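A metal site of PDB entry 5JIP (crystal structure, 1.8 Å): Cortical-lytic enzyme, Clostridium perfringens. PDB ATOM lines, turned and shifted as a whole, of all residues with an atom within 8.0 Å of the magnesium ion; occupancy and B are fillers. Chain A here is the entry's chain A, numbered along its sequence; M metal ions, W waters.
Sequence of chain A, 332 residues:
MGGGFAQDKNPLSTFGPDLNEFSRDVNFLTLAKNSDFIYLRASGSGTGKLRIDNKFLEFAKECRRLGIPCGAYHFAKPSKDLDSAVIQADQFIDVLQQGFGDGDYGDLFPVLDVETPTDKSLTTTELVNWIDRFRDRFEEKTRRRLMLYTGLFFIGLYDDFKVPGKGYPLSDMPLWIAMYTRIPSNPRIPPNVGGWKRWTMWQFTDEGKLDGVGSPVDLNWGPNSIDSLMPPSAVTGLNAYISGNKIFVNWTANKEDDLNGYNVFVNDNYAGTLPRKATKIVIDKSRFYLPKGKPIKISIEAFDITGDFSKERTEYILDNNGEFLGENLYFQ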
ATOM      1  N   ASP A 107       9.749  11.525  25.768  1.00  0.00           N
ATOM      2  CA  ASP A 107      11.117  11.993  25.976  1.00  0.00           C
ATOM      3  C   ASP A 107      12.101  11.252  25.074  1.00  0.00           C
ATOM      4  O   ASP A 107      13.014  11.865  24.507  1.00  0.00           O
ATOM      5  CB  ASP A 107      11.519  11.777  27.422  1.00  0.00           C
ATOM      6  CG  ASP A 107      10.514  12.346  28.398  1.00  0.00           C
ATOM      7  OD1 ASP A 107      10.039  13.478  28.146  1.00  0.00           O
ATOM      8  OD2 ASP A 107      10.251  11.679  29.421  1.00  0.00           O
ATOM      9  N   PHE A 109      13.125   8.542  21.795  1.00  0.00           N
ATOM     10  CA  PHE A 109      12.673   8.240  20.438  1.00  0.00           C
ATOM     11  C   PHE A 109      11.382   7.440  20.509  1.00  0.00           C
ATOM     12  O   PHE A 109      11.361   6.358  21.122  1.00  0.00           O
ATOM     13  CB  PHE A 109      13.670   7.368  19.639  1.00  0.00           C
ATOM     14  CG  PHE A 109      15.014   8.000  19.339  1.00  0.00           C
ATOM     15  CD1 PHE A 109      15.142   9.041  18.425  1.00  0.00           C
ATOM     16  CD2 PHE A 109      16.161   7.464  19.903  1.00  0.00           C
ATOM     17  CE1 PHE A 109      16.379   9.556  18.147  1.00  0.00           C
ATOM     18  CE2 PHE A 109      17.398   7.967  19.604  1.00  0.00           C
ATOM     19  CZ  PHE A 109      17.521   9.003  18.742  1.00  0.00           C
ATOM     20  N   SER A 225      25.097   8.467  26.842  1.00  0.00           N
ATOM     21  CA  SER A 225      24.355   9.560  27.432  1.00  0.00           C
ATOM     22  C   SER A 225      22.869   9.427  27.140  1.00  0.00           C
ATOM     23  O   SER A 225      22.472   9.133  26.011  1.00  0.00           O
ATOM     24  CB  SER A 225      24.818  10.897  26.880  1.00  0.00           C
ATOM     25  OG  SER A 225      24.036  11.935  27.437  1.00  0.00           O
ATOM     26  N   ILE A 226      22.063   9.687  28.162  1.00  0.00           N
ATOM     27  CA  ILE A 226      20.613   9.721  27.991  1.00  0.00           C
ATOM     28  C   ILE A 226      20.228  10.749  26.931  1.00  0.00           C
ATOM     29  O   ILE A 226      19.194  10.618  26.271  1.00  0.00           O
ATOM     30  CB  ILE A 226      19.933  10.007  29.347  1.00  0.00           C
ATOM     31  CG1 ILE A 226      18.422   9.957  29.202  1.00  0.00           C
ATOM     32  CG2 ILE A 226      20.334  11.363  29.901  1.00  0.00           C
ATOM     33  CD1 ILE A 226      17.887   8.520  28.935  1.00  0.00           C
ATOM     34  N   ASP A 227      21.042  11.788  26.758  1.00  0.00           N
ATOM     35  CA  ASP A 227      20.761  12.819  25.774  1.00  0.00           C
ATOM     36  C   ASP A 227      20.651  12.229  24.370  1.00  0.00           C
ATOM     37  O   ASP A 227      19.874  12.739  23.549  1.00  0.00           O
ATOM     38  CB  ASP A 227      21.857  13.895  25.807  1.00  0.00           C
ATOM     39  CG  ASP A 227      21.996  14.599  27.163  1.00  0.00           C
ATOM     40  OD1 ASP A 227      21.049  14.600  27.927  1.00  0.00           O
ATOM     41  OD2 ASP A 227      23.083  15.162  27.423  1.00  0.00           O
ATOM     42  N   SER A 228      21.367  11.136  24.099  1.00  0.00           N
ATOM     43  CA  SER A 228      21.356  10.545  22.759  1.00  0.00           C
ATOM     44  C   SER A 228      20.048   9.821  22.443  1.00  0.00           C
ATOM     45  O   SER A 228      19.860   9.409  21.303  1.00  0.00           O
ATOM     46  CB  SER A 228      22.528   9.574  22.622  1.00  0.00           C
ATOM     47  OG  SER A 228      23.748  10.298  22.667  1.00  0.00           O
ATOM     48  N   LEU A 229      19.169   9.636  23.426  1.00  0.00           N
ATOM     49  CA  LEU A 229      17.836   9.098  23.168  1.00  0.00           C
ATOM     50  C   LEU A 229      16.769  10.179  23.052  1.00  0.00           C
ATOM     51  O   LEU A 229      15.650   9.876  22.602  1.00  0.00           O
ATOM     52  CB  LEU A 229      17.434   8.132  24.305  1.00  0.00           C
ATOM     53  CG  LEU A 229      18.248   6.840  24.442  1.00  0.00           C
ATOM     54  CD1 LEU A 229      17.770   6.039  25.643  1.00  0.00           C
ATOM     55  CD2 LEU A 229      18.160   6.008  23.139  1.00  0.00           C
ATOM     56  N   MET A 230      17.084  11.416  23.466  1.00  0.00           N
ATOM     57  CA  MET A 230      16.108  12.508  23.631  1.00  0.00           C
ATOM     58  C   MET A 230      16.409  13.717  22.746  1.00  0.00           C
ATOM     59  O   MET A 230      17.566  13.969  22.400  1.00  0.00           O
ATOM     60  CB  MET A 230      16.082  12.979  25.089  1.00  0.00           C
ATOM     61  CG  MET A 230      15.850  11.890  26.066  1.00  0.00           C
ATOM     62  SD  MET A 230      15.568  12.482  27.751  1.00  0.00           S
ATOM     63  CE  MET A 230      17.073  13.382  28.114  1.00  0.00           C
ATOM     64  N   PRO A 231      15.397  14.505  22.396  1.00  0.00           N
ATOM     65  CA  PRO A 231      15.669  15.815  21.824  1.00  0.00           C
ATOM     66  C   PRO A 231      16.407  16.681  22.823  1.00  0.00           C
ATOM     67  O   PRO A 231      16.242  16.526  24.059  1.00  0.00           O
ATOM     68  CB  PRO A 231      14.275  16.364  21.516  1.00  0.00           C
ATOM     69  CG  PRO A 231      13.371  15.162  21.529  1.00  0.00           C
ATOM     70  CD  PRO A 231      13.944  14.274  22.529  1.00  0.00           C
ATOM     71  N   PRO A 232      17.177  17.643  22.343  1.00  0.00           N
ATOM     72  CA  PRO A 232      17.792  18.616  23.265  1.00  0.00           C
ATOM     73  C   PRO A 232      16.740  19.470  23.941  1.00  0.00           C
ATOM     74  O   PRO A 232      15.605  19.616  23.469  1.00  0.00           O
ATOM     75  CB  PRO A 232      18.669  19.491  22.350  1.00  0.00           C
ATOM     76  CG  PRO A 232      18.307  19.182  21.022  1.00  0.00           C
ATOM     77  CD  PRO A 232      17.406  18.001  20.941  1.00  0.00           C
ATOM     78  N   SER A 233      17.147  20.056  25.063  1.00  0.00           N
ATOM     79  CA  SER A 233      16.332  21.004  25.802  1.00  0.00           C
ATOM     80  C   SER A 233      16.195  22.321  25.044  1.00  0.00           C
ATOM     81  O   SER A 233      16.965  22.634  24.126  1.00  0.00           O
ATOM     82  CB  SER A 233      16.939  21.314  27.179  1.00  0.00           C
ATOM     83  OG  SER A 233      17.036  20.159  27.992  1.00  0.00           O
ATOM     84  N   GLU A 256      23.901  19.354  26.089  1.00  0.00           N
ATOM     85  CA  GLU A 256      23.738  17.945  25.752  1.00  0.00           C
ATOM     86  C   GLU A 256      24.992  17.361  25.132  1.00  0.00           C
ATOM     87  O   GLU A 256      25.670  17.992  24.298  1.00  0.00           O
ATOM     88  CB  GLU A 256      22.567  17.748  24.797  1.00  0.00           C
ATOM     89  CG  GLU A 256      21.222  17.939  25.424  1.00  0.00           C
ATOM     90  CD  GLU A 256      20.766  19.392  25.420  1.00  0.00           C
ATOM     91  OE1 GLU A 256      21.409  20.241  24.755  1.00  0.00           O
ATOM     92  OE2 GLU A 256      19.749  19.673  26.066  1.00  0.00           O
ATOM     93  N   ASP A 257      25.280  16.106  25.495  1.00  0.00           N
ATOM     94  CA  ASP A 257      26.437  15.416  24.963  1.00  0.00           C
ATOM     95  C   ASP A 257      26.334  15.221  23.473  1.00  0.00           C
ATOM     96  O   ASP A 257      27.352  15.143  22.788  1.00  0.00           O
ATOM     97  CB  ASP A 257      26.605  14.058  25.659  1.00  0.00           C
ATOM     98  CG  ASP A 257      26.767  14.194  27.150  1.00  0.00           C
ATOM     99  OD1 ASP A 257      27.657  14.964  27.548  1.00  0.00           O
ATOM    100  OD2 ASP A 257      25.980  13.593  27.926  1.00  0.00           O
ATOM    101  N   ASP A 258      25.113  15.154  22.939  1.00  0.00           N
ATOM    102  CA  ASP A 258      24.907  14.933  21.522  1.00  0.00           C
ATOM    103  C   ASP A 258      24.499  16.202  20.803  1.00  0.00           C
ATOM    104  O   ASP A 258      23.935  16.130  19.706  1.00  0.00           O
ATOM    105  CB  ASP A 258      23.857  13.835  21.294  1.00  0.00           C
ATOM    106  CG  ASP A 258      22.489  14.227  21.821  1.00  0.00           C
ATOM    107  OD1 ASP A 258      22.400  15.152  22.683  1.00  0.00           O
ATOM    108  OD2 ASP A 258      21.477  13.593  21.420  1.00  0.00           O
ATOM    109  N   LEU A 259      24.715  17.367  21.419  1.00  0.00           N
ATOM    110  CA  LEU A 259      24.391  18.634  20.781  1.00  0.00           C
ATOM    111  C   LEU A 259      25.127  18.756  19.448  1.00  0.00           C
ATOM    112  O   LEU A 259      26.304  18.429  19.330  1.00  0.00           O
ATOM    113  CB  LEU A 259      24.766  19.787  21.691  1.00  0.00           C
ATOM    114  CG  LEU A 259      24.433  21.179  21.182  1.00  0.00           C
ATOM    115  CD1 LEU A 259      22.947  21.396  21.140  1.00  0.00           C
ATOM    116  CD2 LEU A 259      25.143  22.170  22.061  1.00  0.00           C
ATOM    117  N   PHE A 303      19.541  21.475  18.043  1.00  0.00           N
ATOM    118  CA  PHE A 303      19.288  20.152  17.474  1.00  0.00           C
ATOM    119  C   PHE A 303      20.489  19.256  17.764  1.00  0.00           C
ATOM    120  O   PHE A 303      21.597  19.742  18.024  1.00  0.00           O
ATOM    121  CB  PHE A 303      18.973  20.182  15.948  1.00  0.00           C
ATOM    122  CG  PHE A 303      20.026  20.835  15.078  1.00  0.00           C
ATOM    123  CD1 PHE A 303      21.115  20.103  14.588  1.00  0.00           C
ATOM    124  CD2 PHE A 303      19.900  22.156  14.692  1.00  0.00           C
ATOM    125  CE1 PHE A 303      22.067  20.707  13.771  1.00  0.00           C
ATOM    126  CE2 PHE A 303      20.821  22.762  13.865  1.00  0.00           C
ATOM    127  CZ  PHE A 303      21.921  22.046  13.399  1.00  0.00           C
ATOM    128  N   ASP A 304      20.246  17.949  17.766  1.00  0.00           N
ATOM    129  CA  ASP A 304      21.264  16.984  18.178  1.00  0.00           C
ATOM    130  C   ASP A 304      21.728  16.159  16.971  1.00  0.00           C
ATOM    131  O   ASP A 304      21.275  16.348  15.847  1.00  0.00           O
ATOM    132  CB  ASP A 304      20.760  16.121  19.341  1.00  0.00           C
ATOM    133  CG  ASP A 304      19.557  15.252  18.991  1.00  0.00           C
ATOM    134  OD1 ASP A 304      19.241  15.052  17.800  1.00  0.00           O
ATOM    135  OD2 ASP A 304      18.923  14.749  19.950  1.00  0.00           O
ATOM    136  N   ILE A 305      22.704  15.277  17.208  1.00  0.00           N
ATOM    137  CA  ILE A 305      23.393  14.601  16.122  1.00  0.00           C
ATOM    138  C   ILE A 305      22.443  13.804  15.252  1.00  0.00           C
ATOM    139  O   ILE A 305      22.647  13.713  14.038  1.00  0.00           O
ATOM    140  CB  ILE A 305      24.522  13.721  16.694  1.00  0.00           C
ATOM    141  CG1 ILE A 305      25.596  14.638  17.274  1.00  0.00           C
ATOM    142  CG2 ILE A 305      25.112  12.815  15.605  1.00  0.00           C
ATOM    143  CD1 ILE A 305      26.690  13.888  18.050  1.00  0.00           C
ATOM    144  N   THR A 306      21.400  13.223  15.828  1.00  0.00           N
ATOM    145  CA  THR A 306      20.499  12.404  15.027  1.00  0.00           C
ATOM    146  C   THR A 306      19.279  13.181  14.557  1.00  0.00           C
ATOM    147  O   THR A 306      18.375  12.594  13.978  1.00  0.00           O
ATOM    148  CB  THR A 306      20.117  11.111  15.794  1.00  0.00           C
ATOM    149  OG1 THR A 306      19.812  11.403  17.157  1.00  0.00           O
ATOM    150  CG2 THR A 306      21.304  10.147  15.777  1.00  0.00           C
ATOM    151  N   GLY A 307      19.258  14.498  14.731  1.00  0.00           N
ATOM    152  CA  GLY A 307      18.302  15.318  14.008  1.00  0.00           C
ATOM    153  C   GLY A 307      17.004  15.612  14.709  1.00  0.00           C
ATOM    154  O   GLY A 307      16.019  15.956  14.037  1.00  0.00           O
ATOM    155  N   ASP A 308      16.939  15.491  16.040  1.00  0.00           N
ATOM    156  CA  ASP A 308      15.834  16.024  16.817  1.00  0.00           C
ATOM    157  C   ASP A 308      16.122  17.429  17.310  1.00  0.00           C
ATOM    158  O   ASP A 308      17.281  17.827  17.516  1.00  0.00           O
ATOM    159  CB  ASP A 308      15.526  15.118  18.014  1.00  0.00           C
ATOM    160  CG  ASP A 308      14.722  13.881  17.608  1.00  0.00           C
ATOM    161  OD1 ASP A 308      13.706  14.021  16.933  1.00  0.00           O
ATOM    162  OD2 ASP A 308      15.142  12.759  17.957  1.00  0.00           O
ATOM    163  N   PHE A 309      15.052  18.175  17.521  1.00  0.00           N
ATOM    164  CA  PHE A 309      15.075  19.586  17.885  1.00  0.00           C
ATOM    165  C   PHE A 309      14.476  19.831  19.259  1.00  0.00           C
ATOM    166  O   PHE A 309      13.663  19.047  19.760  1.00  0.00           O
ATOM    167  CB  PHE A 309      14.298  20.404  16.873  1.00  0.00           C
ATOM    168  CG  PHE A 309      14.724  20.147  15.475  1.00  0.00           C
ATOM    169  CD1 PHE A 309      14.179  19.102  14.768  1.00  0.00           C
ATOM    170  CD2 PHE A 309      15.698  20.917  14.890  1.00  0.00           C
ATOM    171  CE1 PHE A 309      14.587  18.851  13.458  1.00  0.00           C
ATOM    172  CE2 PHE A 309      16.127  20.643  13.599  1.00  0.00           C
ATOM    173  CZ  PHE A 309      15.559  19.602  12.894  1.00  0.00           C
HETATM  174 MG    MG M   1      19.477  13.821  21.725  1.00  0.00          MG
HETATM  175  O   HOH W   1      19.021  12.126  20.577  1.00  0.00           O
HETATM  176  O   HOH W   2      19.825  15.629  22.812  1.00  0.00           O
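OD1 of Asp 304 is in hydrogen-bond range of N of Gly 307, at 3.1 Å. OD2 of Asp 227 lies within hydrogen-bond range of N of Asp 257. N of Thr 306 lies close to OD1 of Asp 304. The backbone carbonyl oxygen (O) of Asp 258 lies within hydrogen-bond range of the backbone NH (N) of Ile 305. N of Asp 227 lies close to OG of Ser 225, at 3.1 Å. The backbone NH of Asp 308 sits at hydrogen-bond distance from the side-chain carboxylate of Asp 304 (2.9 Å).
Ser 228 touches the magnesium ion. Five residues have an atom within 4 Å of the magnesium ion: Asp 227, Ser 228, Met 230, Asp 258 and Asp 304.
The magnesium ion is bound by the backbone carbonyl oxygen of Met 230, the side-chain carboxylate of Asp 258, the side-chain carboxylate of Asp 304, water W1, water W2 and the backbone carbonyl oxygen of Asp 227. The magnesium ion has six donor atoms within binding distance.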
